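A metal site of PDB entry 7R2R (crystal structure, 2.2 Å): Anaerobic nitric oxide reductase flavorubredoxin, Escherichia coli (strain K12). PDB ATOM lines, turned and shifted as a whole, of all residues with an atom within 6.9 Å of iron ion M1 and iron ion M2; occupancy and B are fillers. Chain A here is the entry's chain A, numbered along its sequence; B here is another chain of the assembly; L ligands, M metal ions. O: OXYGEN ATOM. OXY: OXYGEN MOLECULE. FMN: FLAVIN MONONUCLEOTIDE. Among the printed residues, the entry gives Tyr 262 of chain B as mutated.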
ATOM      1  N   PHE A  22      -3.531 -22.491   2.362  1.00  0.00           N
ATOM      2  CA  PHE A  22      -4.154 -23.621   1.678  1.00  0.00           C
ATOM      3  C   PHE A  22      -3.485 -24.922   2.092  1.00  0.00           C
ATOM      4  O   PHE A  22      -2.310 -24.929   2.458  1.00  0.00           O
ATOM      5  CB  PHE A  22      -4.094 -23.450   0.161  1.00  0.00           C
ATOM      6  CG  PHE A  22      -5.371 -22.949  -0.450  1.00  0.00           C
ATOM      7  CD1 PHE A  22      -5.609 -21.603  -0.615  1.00  0.00           C
ATOM      8  CD2 PHE A  22      -6.344 -23.850  -0.872  1.00  0.00           C
ATOM      9  CE1 PHE A  22      -6.784 -21.140  -1.183  1.00  0.00           C
ATOM     10  CE2 PHE A  22      -7.526 -23.400  -1.438  1.00  0.00           C
ATOM     11  CZ  PHE A  22      -7.750 -22.042  -1.586  1.00  0.00           C
ATOM     12  N   HIS A  23      -4.240 -26.022   2.024  1.00  0.00           N
ATOM     13  CA  HIS A  23      -3.753 -27.335   2.458  1.00  0.00           C
ATOM     14  C   HIS A  23      -3.228 -27.259   3.880  1.00  0.00           C
ATOM     15  O   HIS A  23      -2.100 -27.682   4.156  1.00  0.00           O
ATOM     16  CB  HIS A  23      -2.671 -27.862   1.515  1.00  0.00           C
ATOM     17  CG  HIS A  23      -3.111 -27.952   0.089  1.00  0.00           C
ATOM     18  ND1 HIS A  23      -2.217 -28.094  -0.962  1.00  0.00           N
ATOM     19  CD2 HIS A  23      -4.344 -27.929  -0.469  1.00  0.00           C
ATOM     20  CE1 HIS A  23      -2.890 -28.157  -2.097  1.00  0.00           C
ATOM     21  NE2 HIS A  23      -4.173 -28.051  -1.830  1.00  0.00           N
ATOM     22  N   SER A  34      -9.337 -17.248  -5.953  1.00  0.00           N
ATOM     23  CA  SER A  34     -10.741 -17.199  -6.332  1.00  0.00           C
ATOM     24  C   SER A  34     -11.275 -18.605  -6.538  1.00  0.00           C
ATOM     25  O   SER A  34     -10.524 -19.534  -6.861  1.00  0.00           O
ATOM     26  CB  SER A  34     -10.929 -16.364  -7.604  1.00  0.00           C
ATOM     27  OG  SER A  34     -10.356 -17.018  -8.726  1.00  0.00           O
ATOM     28  N   TYR A  35     -12.578 -18.770  -6.343  1.00  0.00           N
ATOM     29  CA  TYR A  35     -13.230 -20.055  -6.549  1.00  0.00           C
ATOM     30  C   TYR A  35     -14.299 -19.892  -7.608  1.00  0.00           C
ATOM     31  O   TYR A  35     -15.403 -19.418  -7.319  1.00  0.00           O
ATOM     32  CB  TYR A  35     -13.810 -20.577  -5.240  1.00  0.00           C
ATOM     33  CG  TYR A  35     -12.899 -20.347  -4.052  1.00  0.00           C
ATOM     34  CD1 TYR A  35     -11.730 -21.074  -3.906  1.00  0.00           C
ATOM     35  CD2 TYR A  35     -13.194 -19.384  -3.102  1.00  0.00           C
ATOM     36  CE1 TYR A  35     -10.882 -20.854  -2.834  1.00  0.00           C
ATOM     37  CE2 TYR A  35     -12.371 -19.161  -2.030  1.00  0.00           C
ATOM     38  CZ  TYR A  35     -11.211 -19.901  -1.892  1.00  0.00           C
ATOM     39  OH  TYR A  35     -10.379 -19.675  -0.823  1.00  0.00           O
ATOM     40  N   HIS A  79     -14.737 -31.796  -9.562  1.00  0.00           N
ATOM     41  CA  HIS A  79     -13.772 -32.015  -8.506  1.00  0.00           C
ATOM     42  C   HIS A  79     -14.416 -31.752  -7.150  1.00  0.00           C
ATOM     43  O   HIS A  79     -15.013 -30.694  -6.948  1.00  0.00           O
ATOM     44  CB  HIS A  79     -12.555 -31.103  -8.723  1.00  0.00           C
ATOM     45  CG  HIS A  79     -11.411 -31.368  -7.786  1.00  0.00           C
ATOM     46  ND1 HIS A  79     -11.023 -32.629  -7.407  1.00  0.00           N
ATOM     47  CD2 HIS A  79     -10.561 -30.514  -7.165  1.00  0.00           C
ATOM     48  CE1 HIS A  79      -9.994 -32.557  -6.588  1.00  0.00           C
ATOM     49  NE2 HIS A  79      -9.690 -31.273  -6.425  1.00  0.00           N
ATOM     50  N   GLU A  81     -13.115 -31.485  -4.065  1.00  0.00           N
ATOM     51  CA  GLU A  81     -12.325 -30.899  -2.992  1.00  0.00           C
ATOM     52  C   GLU A  81     -13.101 -29.740  -2.398  1.00  0.00           C
ATOM     53  O   GLU A  81     -13.854 -29.057  -3.093  1.00  0.00           O
ATOM     54  CB  GLU A  81     -10.952 -30.445  -3.502  1.00  0.00           C
ATOM     55  CG  GLU A  81      -9.963 -30.097  -2.404  1.00  0.00           C
ATOM     56  CD  GLU A  81      -8.534 -29.992  -2.902  1.00  0.00           C
ATOM     57  OE1 GLU A  81      -8.288 -30.204  -4.104  1.00  0.00           O
ATOM     58  OE2 GLU A  81      -7.632 -29.694  -2.084  1.00  0.00           O
ATOM     59  N   ASP A  83     -12.796 -26.785  -1.669  1.00  0.00           N
ATOM     60  CA  ASP A  83     -12.761 -25.433  -2.225  1.00  0.00           C
ATOM     61  C   ASP A  83     -13.618 -25.299  -3.480  1.00  0.00           C
ATOM     62  O   ASP A  83     -13.702 -24.218  -4.068  1.00  0.00           O
ATOM     63  CB  ASP A  83     -11.313 -25.026  -2.530  1.00  0.00           C
ATOM     64  CG  ASP A  83     -10.636 -25.963  -3.504  1.00  0.00           C
ATOM     65  OD1 ASP A  83     -10.952 -27.179  -3.475  1.00  0.00           O
ATOM     66  OD2 ASP A  83      -9.791 -25.494  -4.297  1.00  0.00           O
ATOM     67  N   HIS A  84     -14.249 -26.387  -3.899  1.00  0.00           N
ATOM     68  CA  HIS A  84     -15.104 -26.362  -5.086  1.00  0.00           C
ATOM     69  C   HIS A  84     -16.461 -27.008  -4.830  1.00  0.00           C
ATOM     70  O   HIS A  84     -17.440 -26.696  -5.497  1.00  0.00           O
ATOM     71  CB  HIS A  84     -14.410 -27.051  -6.258  1.00  0.00           C
ATOM     72  CG  HIS A  84     -13.028 -26.556  -6.521  1.00  0.00           C
ATOM     73  ND1 HIS A  84     -12.750 -25.252  -6.854  1.00  0.00           N
ATOM     74  CD2 HIS A  84     -11.834 -27.200  -6.490  1.00  0.00           C
ATOM     75  CE1 HIS A  84     -11.451 -25.104  -7.017  1.00  0.00           C
ATOM     76  NE2 HIS A  84     -10.871 -26.268  -6.808  1.00  0.00           N
ATOM     77  N   HIS A 147      -5.764 -33.357 -10.086  1.00  0.00           N
ATOM     78  CA  HIS A 147      -4.756 -33.984  -9.233  1.00  0.00           C
ATOM     79  C   HIS A 147      -5.354 -35.049  -8.314  1.00  0.00           C
ATOM     80  O   HIS A 147      -4.672 -35.622  -7.476  1.00  0.00           O
ATOM     81  CB  HIS A 147      -4.025 -32.921  -8.401  1.00  0.00           C
ATOM     82  CG  HIS A 147      -4.923 -32.180  -7.467  1.00  0.00           C
ATOM     83  ND1 HIS A 147      -5.123 -32.563  -6.154  1.00  0.00           N
ATOM     84  CD2 HIS A 147      -5.688 -31.073  -7.648  1.00  0.00           C
ATOM     85  CE1 HIS A 147      -5.958 -31.722  -5.575  1.00  0.00           C
ATOM     86  NE2 HIS A 147      -6.323 -30.818  -6.458  1.00  0.00           N
ATOM     87  N   TRP A 148      -6.655 -35.305  -8.481  1.00  0.00           N
ATOM     88  CA  TRP A 148      -7.357 -36.289  -7.656  1.00  0.00           C
ATOM     89  C   TRP A 148      -7.932 -37.401  -8.521  1.00  0.00           C
ATOM     90  O   TRP A 148      -8.084 -37.241  -9.736  1.00  0.00           O
ATOM     91  CB  TRP A 148      -8.472 -35.618  -6.854  1.00  0.00           C
ATOM     92  CG  TRP A 148      -8.060 -35.128  -5.492  1.00  0.00           C
ATOM     93  CD1 TRP A 148      -6.788 -34.934  -5.047  1.00  0.00           C
ATOM     94  CD2 TRP A 148      -8.920 -34.780  -4.401  1.00  0.00           C
ATOM     95  NE1 TRP A 148      -6.801 -34.478  -3.753  1.00  0.00           N
ATOM     96  CE2 TRP A 148      -8.102 -34.376  -3.328  1.00  0.00           C
ATOM     97  CE3 TRP A 148     -10.314 -34.768  -4.224  1.00  0.00           C
ATOM     98  CZ2 TRP A 148      -8.623 -33.972  -2.100  1.00  0.00           C
ATOM     99  CZ3 TRP A 148     -10.827 -34.369  -3.011  1.00  0.00           C
ATOM    100  CH2 TRP A 148      -9.980 -33.973  -1.961  1.00  0.00           C
ATOM    101  N   SER A 151     -11.090 -36.235 -10.429  1.00  0.00           N
ATOM    102  CA  SER A 151     -10.972 -35.074 -11.299  1.00  0.00           C
ATOM    103  C   SER A 151     -11.423 -35.338 -12.730  1.00  0.00           C
ATOM    104  O   SER A 151     -11.164 -36.409 -13.293  1.00  0.00           O
ATOM    105  CB  SER A 151      -9.531 -34.565 -11.305  1.00  0.00           C
ATOM    106  OG  SER A 151      -9.116 -34.215  -9.995  1.00  0.00           O
ATOM    107  N   ASN A 165     -11.403 -26.955 -14.354  1.00  0.00           N
ATOM    108  CA  ASN A 165     -11.291 -26.960 -12.898  1.00  0.00           C
ATOM    109  C   ASN A 165      -9.897 -26.523 -12.445  1.00  0.00           C
ATOM    110  O   ASN A 165      -9.427 -25.464 -12.837  1.00  0.00           O
ATOM    111  CB  ASN A 165     -11.645 -28.344 -12.344  1.00  0.00           C
ATOM    112  CG  ASN A 165     -12.002 -28.307 -10.869  1.00  0.00           C
ATOM    113  OD1 ASN A 165     -11.163 -28.574 -10.013  1.00  0.00           O
ATOM    114  ND2 ASN A 165     -13.261 -27.974 -10.567  1.00  0.00           N
ATOM    115  N   ASP A 166      -9.237 -27.346 -11.634  1.00  0.00           N
ATOM    116  CA  ASP A 166      -7.924 -27.010 -11.079  1.00  0.00           C
ATOM    117  C   ASP A 166      -6.843 -26.838 -12.145  1.00  0.00           C
ATOM    118  O   ASP A 166      -5.954 -25.996 -12.006  1.00  0.00           O
ATOM    119  CB  ASP A 166      -7.470 -28.077 -10.079  1.00  0.00           C
ATOM    120  CG  ASP A 166      -8.019 -27.843  -8.687  1.00  0.00           C
ATOM    121  OD1 ASP A 166      -8.531 -26.737  -8.419  1.00  0.00           O
ATOM    122  OD2 ASP A 166      -7.918 -28.762  -7.849  1.00  0.00           O
ATOM    123  N   HIS A 171      -3.727 -19.469  -8.057  1.00  0.00           N
ATOM    124  CA  HIS A 171      -4.236 -18.687  -6.933  1.00  0.00           C
ATOM    125  C   HIS A 171      -3.876 -17.213  -7.107  1.00  0.00           C
ATOM    126  O   HIS A 171      -2.838 -16.751  -6.627  1.00  0.00           O
ATOM    127  CB  HIS A 171      -3.705 -19.222  -5.611  1.00  0.00           C
ATOM    128  CG  HIS A 171      -4.173 -20.618  -5.303  1.00  0.00           C
ATOM    129  ND1 HIS A 171      -5.492 -20.931  -5.099  1.00  0.00           N
ATOM    130  CD2 HIS A 171      -3.486 -21.775  -5.169  1.00  0.00           C
ATOM    131  CE1 HIS A 171      -5.612 -22.220  -4.850  1.00  0.00           C
ATOM    132  NE2 HIS A 171      -4.405 -22.761  -4.883  1.00  0.00           N
ATOM    133  N   TYR A 194       1.841 -22.699  -8.719  1.00  0.00           N
ATOM    134  CA  TYR A 194       0.764 -23.672  -8.562  1.00  0.00           C
ATOM    135  C   TYR A 194       1.163 -25.051  -9.059  1.00  0.00           C
ATOM    136  O   TYR A 194       0.949 -26.047  -8.378  1.00  0.00           O
ATOM    137  CB  TYR A 194      -0.486 -23.181  -9.293  1.00  0.00           C
ATOM    138  CG  TYR A 194      -1.707 -24.053  -9.073  1.00  0.00           C
ATOM    139  CD1 TYR A 194      -2.035 -25.065  -9.967  1.00  0.00           C
ATOM    140  CD2 TYR A 194      -2.535 -23.857  -7.970  1.00  0.00           C
ATOM    141  CE1 TYR A 194      -3.144 -25.863  -9.766  1.00  0.00           C
ATOM    142  CE2 TYR A 194      -3.647 -24.646  -7.767  1.00  0.00           C
ATOM    143  CZ  TYR A 194      -3.949 -25.647  -8.672  1.00  0.00           C
ATOM    144  OH  TYR A 194      -5.062 -26.436  -8.470  1.00  0.00           O
ATOM    145  N   ILE A 198       1.945 -28.477  -6.646  1.00  0.00           N
ATOM    146  CA  ILE A 198       0.763 -29.337  -6.700  1.00  0.00           C
ATOM    147  C   ILE A 198       0.866 -30.467  -7.733  1.00  0.00           C
ATOM    148  O   ILE A 198       0.638 -31.624  -7.412  1.00  0.00           O
ATOM    149  CB  ILE A 198      -0.516 -28.533  -6.991  1.00  0.00           C
ATOM    150  CG1 ILE A 198      -0.662 -27.366  -6.004  1.00  0.00           C
ATOM    151  CG2 ILE A 198      -1.744 -29.424  -6.963  1.00  0.00           C
ATOM    152  CD1 ILE A 198      -0.645 -27.797  -4.565  1.00  0.00           C
ATOM    153  N   SER A 226     -11.034 -23.247 -12.292  1.00  0.00           N
ATOM    154  CA  SER A 226     -11.737 -23.093 -11.026  1.00  0.00           C
ATOM    155  C   SER A 226     -11.001 -22.107 -10.115  1.00  0.00           C
ATOM    156  O   SER A 226     -11.521 -21.710  -9.072  1.00  0.00           O
ATOM    157  CB  SER A 226     -11.887 -24.447 -10.326  1.00  0.00           C
ATOM    158  OG  SER A 226     -10.617 -24.976  -9.973  1.00  0.00           O
ATOM    159  N   HIS A 227      -9.794 -21.718 -10.529  1.00  0.00           N
ATOM    160  CA  HIS A 227      -8.980 -20.775  -9.759  1.00  0.00           C
ATOM    161  C   HIS A 227      -8.380 -19.694 -10.656  1.00  0.00           C
ATOM    162  O   HIS A 227      -7.680 -20.003 -11.616  1.00  0.00           O
ATOM    163  CB  HIS A 227      -7.859 -21.495  -9.010  1.00  0.00           C
ATOM    164  CG  HIS A 227      -8.327 -22.360  -7.895  1.00  0.00           C
ATOM    165  ND1 HIS A 227      -8.987 -21.871  -6.791  1.00  0.00           N
ATOM    166  CD2 HIS A 227      -8.214 -23.701  -7.690  1.00  0.00           C
ATOM    167  CE1 HIS A 227      -9.266 -22.853  -5.964  1.00  0.00           C
ATOM    168  NE2 HIS A 227      -8.806 -23.982  -6.483  1.00  0.00           N
ATOM    169  N   TYR B 262      -7.998 -30.247   6.159  1.00  0.00           N
ATOM    170  CA  TYR B 262      -9.438 -30.008   6.129  1.00  0.00           C
ATOM    171  C   TYR B 262     -10.135 -30.476   7.401  1.00  0.00           C
ATOM    172  O   TYR B 262     -11.326 -30.777   7.382  1.00  0.00           O
ATOM    173  CB  TYR B 262     -10.061 -30.692   4.907  1.00  0.00           C
ATOM    174  CG  TYR B 262      -9.523 -30.184   3.593  1.00  0.00           C
ATOM    175  CD1 TYR B 262      -9.781 -28.883   3.175  1.00  0.00           C
ATOM    176  CD2 TYR B 262      -8.743 -30.999   2.779  1.00  0.00           C
ATOM    177  CE1 TYR B 262      -9.297 -28.415   1.977  1.00  0.00           C
ATOM    178  CE2 TYR B 262      -8.245 -30.524   1.565  1.00  0.00           C
ATOM    179  CZ  TYR B 262      -8.522 -29.234   1.176  1.00  0.00           C
ATOM    180  OH  TYR B 262      -8.041 -28.757  -0.020  1.00  0.00           O
HETATM  181  O     O L   1      -9.321 -28.013  -5.381  1.00  0.00           O
HETATM  182  O1  OXY L   2      -5.770 -27.251  -5.742  1.00  0.00           O
HETATM  183  O2  OXY L   2      -6.522 -26.325  -5.905  1.00  0.00           O
HETATM  184  N1  FMN L   3      -5.179 -39.089  -0.059  1.00  0.00           N
HETATM  185  C2  FMN L   3      -4.531 -40.302  -0.205  1.00  0.00           C
HETATM  186  O2  FMN L   3      -5.076 -41.339   0.165  1.00  0.00           O
HETATM  187  N3  FMN L   3      -3.269 -40.357  -0.773  1.00  0.00           N
HETATM  188  C4  FMN L   3      -2.655 -39.192  -1.185  1.00  0.00           C
HETATM  189  O4  FMN L   3      -1.532 -39.251  -1.698  1.00  0.00           O
HETATM  190  C4A FMN L   3      -3.295 -37.976  -1.043  1.00  0.00           C
HETATM  191  N5  FMN L   3      -2.685 -36.810  -1.464  1.00  0.00           N
HETATM  192  C5A FMN L   3      -3.329 -35.599  -1.310  1.00  0.00           C
HETATM  193  C6  FMN L   3      -2.711 -34.429  -1.734  1.00  0.00           C
HETATM  194  C7  FMN L   3      -3.346 -33.214  -1.583  1.00  0.00           C
HETATM  195  C7M FMN L   3      -2.667 -31.952  -2.049  1.00  0.00           C
HETATM  196  C8  FMN L   3      -4.615 -33.148  -1.022  1.00  0.00           C
HETATM  197  C8M FMN L   3      -5.319 -31.840  -0.860  1.00  0.00           C
HETATM  198  C9  FMN L   3      -5.234 -34.318  -0.597  1.00  0.00           C
HETATM  199  C9A FMN L   3      -4.600 -35.546  -0.738  1.00  0.00           C
HETATM  200  N10 FMN L   3      -5.210 -36.712  -0.317  1.00  0.00           N
HETATM  201  C10 FMN L   3      -4.565 -37.924  -0.471  1.00  0.00           C
HETATM  202  C1' FMN L   3      -6.582 -36.681   0.296  1.00  0.00           C
HETATM  203  C2' FMN L   3      -6.547 -36.399   1.798  1.00  0.00           C
HETATM  204  O2' FMN L   3      -5.744 -37.348   2.458  1.00  0.00           O
HETATM  205  C3' FMN L   3      -7.974 -36.428   2.354  1.00  0.00           C
HETATM  206  O3' FMN L   3      -8.676 -35.298   1.879  1.00  0.00           O
HETATM  207  C4' FMN L   3      -8.003 -36.432   3.889  1.00  0.00           C
HETATM  208  O4' FMN L   3      -9.213 -36.997   4.316  1.00  0.00           O
HETATM  209  C5' FMN L   3      -7.877 -35.030   4.465  1.00  0.00           C
HETATM  210  O5' FMN L   3      -7.217 -35.088   5.707  1.00  0.00           O
HETATM  211  P   FMN L   3      -7.186 -33.833   6.714  1.00  0.00           P
HETATM  212  O1P FMN L   3      -7.075 -34.354   8.121  1.00  0.00           O
HETATM  213  O2P FMN L   3      -6.010 -32.955   6.382  1.00  0.00           O
HETATM  214  O3P FMN L   3      -8.472 -33.052   6.587  1.00  0.00           O
HETATM  215 FE    FE M   1      -7.948 -29.619  -6.004  1.00  0.00          FE
HETATM  216 FE    FE M   2      -8.905 -26.117  -6.094  1.00  0.00          FE
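The backbone NH (N) of Asp 166 sits at hydrogen-bond distance from the side-chain hydroxyl (OG) of Ser 226.
The side-chain hydroxyl (OH) of Tyr 194 sits close to the side-chain carboxylate (OD1) of Asp 166, 3.5 Å away.
The indole nitrogen (NE1) of Trp 148 lies close to a ring nitrogen (ND1) of His 147, at 3.5 Å.
N of His 147 is in hydrogen-bond range of OG of Ser 151, 3.5 Å away.
OG of Ser 226 sits close to NE2 of His 84.
The backbone carbonyl oxygen (O) of Ser 34 sits at hydrogen-bond distance from a ring nitrogen (ND1) of His 227, 2.8 Å away.
Iron ion M1 is bound by the side-chain carboxylate of Glu 81 (2.0 Å), the side-chain carboxylate of Asp 166 (2.0 Å), a ring nitrogen (NE2) of His 147 (2.1 Å), an oxygen (O) of O L1 (2.2 Å) and a ring nitrogen (NE2) of His 79 (2.4 Å).
Iron ion M1 has five donor atoms within binding distance.
OH of Tyr 194 lies within hydrogen-bond range of O1 of OXY L2 (2.9 Å).
The backbone NH of Tyr 262 of chain B lies within hydrogen-bond range of an oxygen (O3P) of FMN L3 (2.9 Å).
Of the 19 residues printed, 4 come within 4 Å of iron ion M1.
Iron ion M2 is bound by an oxygen (O) of O L1 (2.1 Å), a ring nitrogen (NE2) of His 84 (2.1 Å), the side-chain carboxylate (OD2) of Asp 83 (2.1 Å), a ring nitrogen (NE2) of His 227 (2.2 Å), an oxygen (O2) of OXY L2 (2.4 Å) and the side-chain carboxylate (OD1) of Asp 166 (2.4 Å).
Four residues have an atom within 4 Å of iron ion M2: Asp 83, His 84, Asp 166 and His 227.
The nearest printed residue that does not touch iron ion M2 is Ser 226 (4.4 Å).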
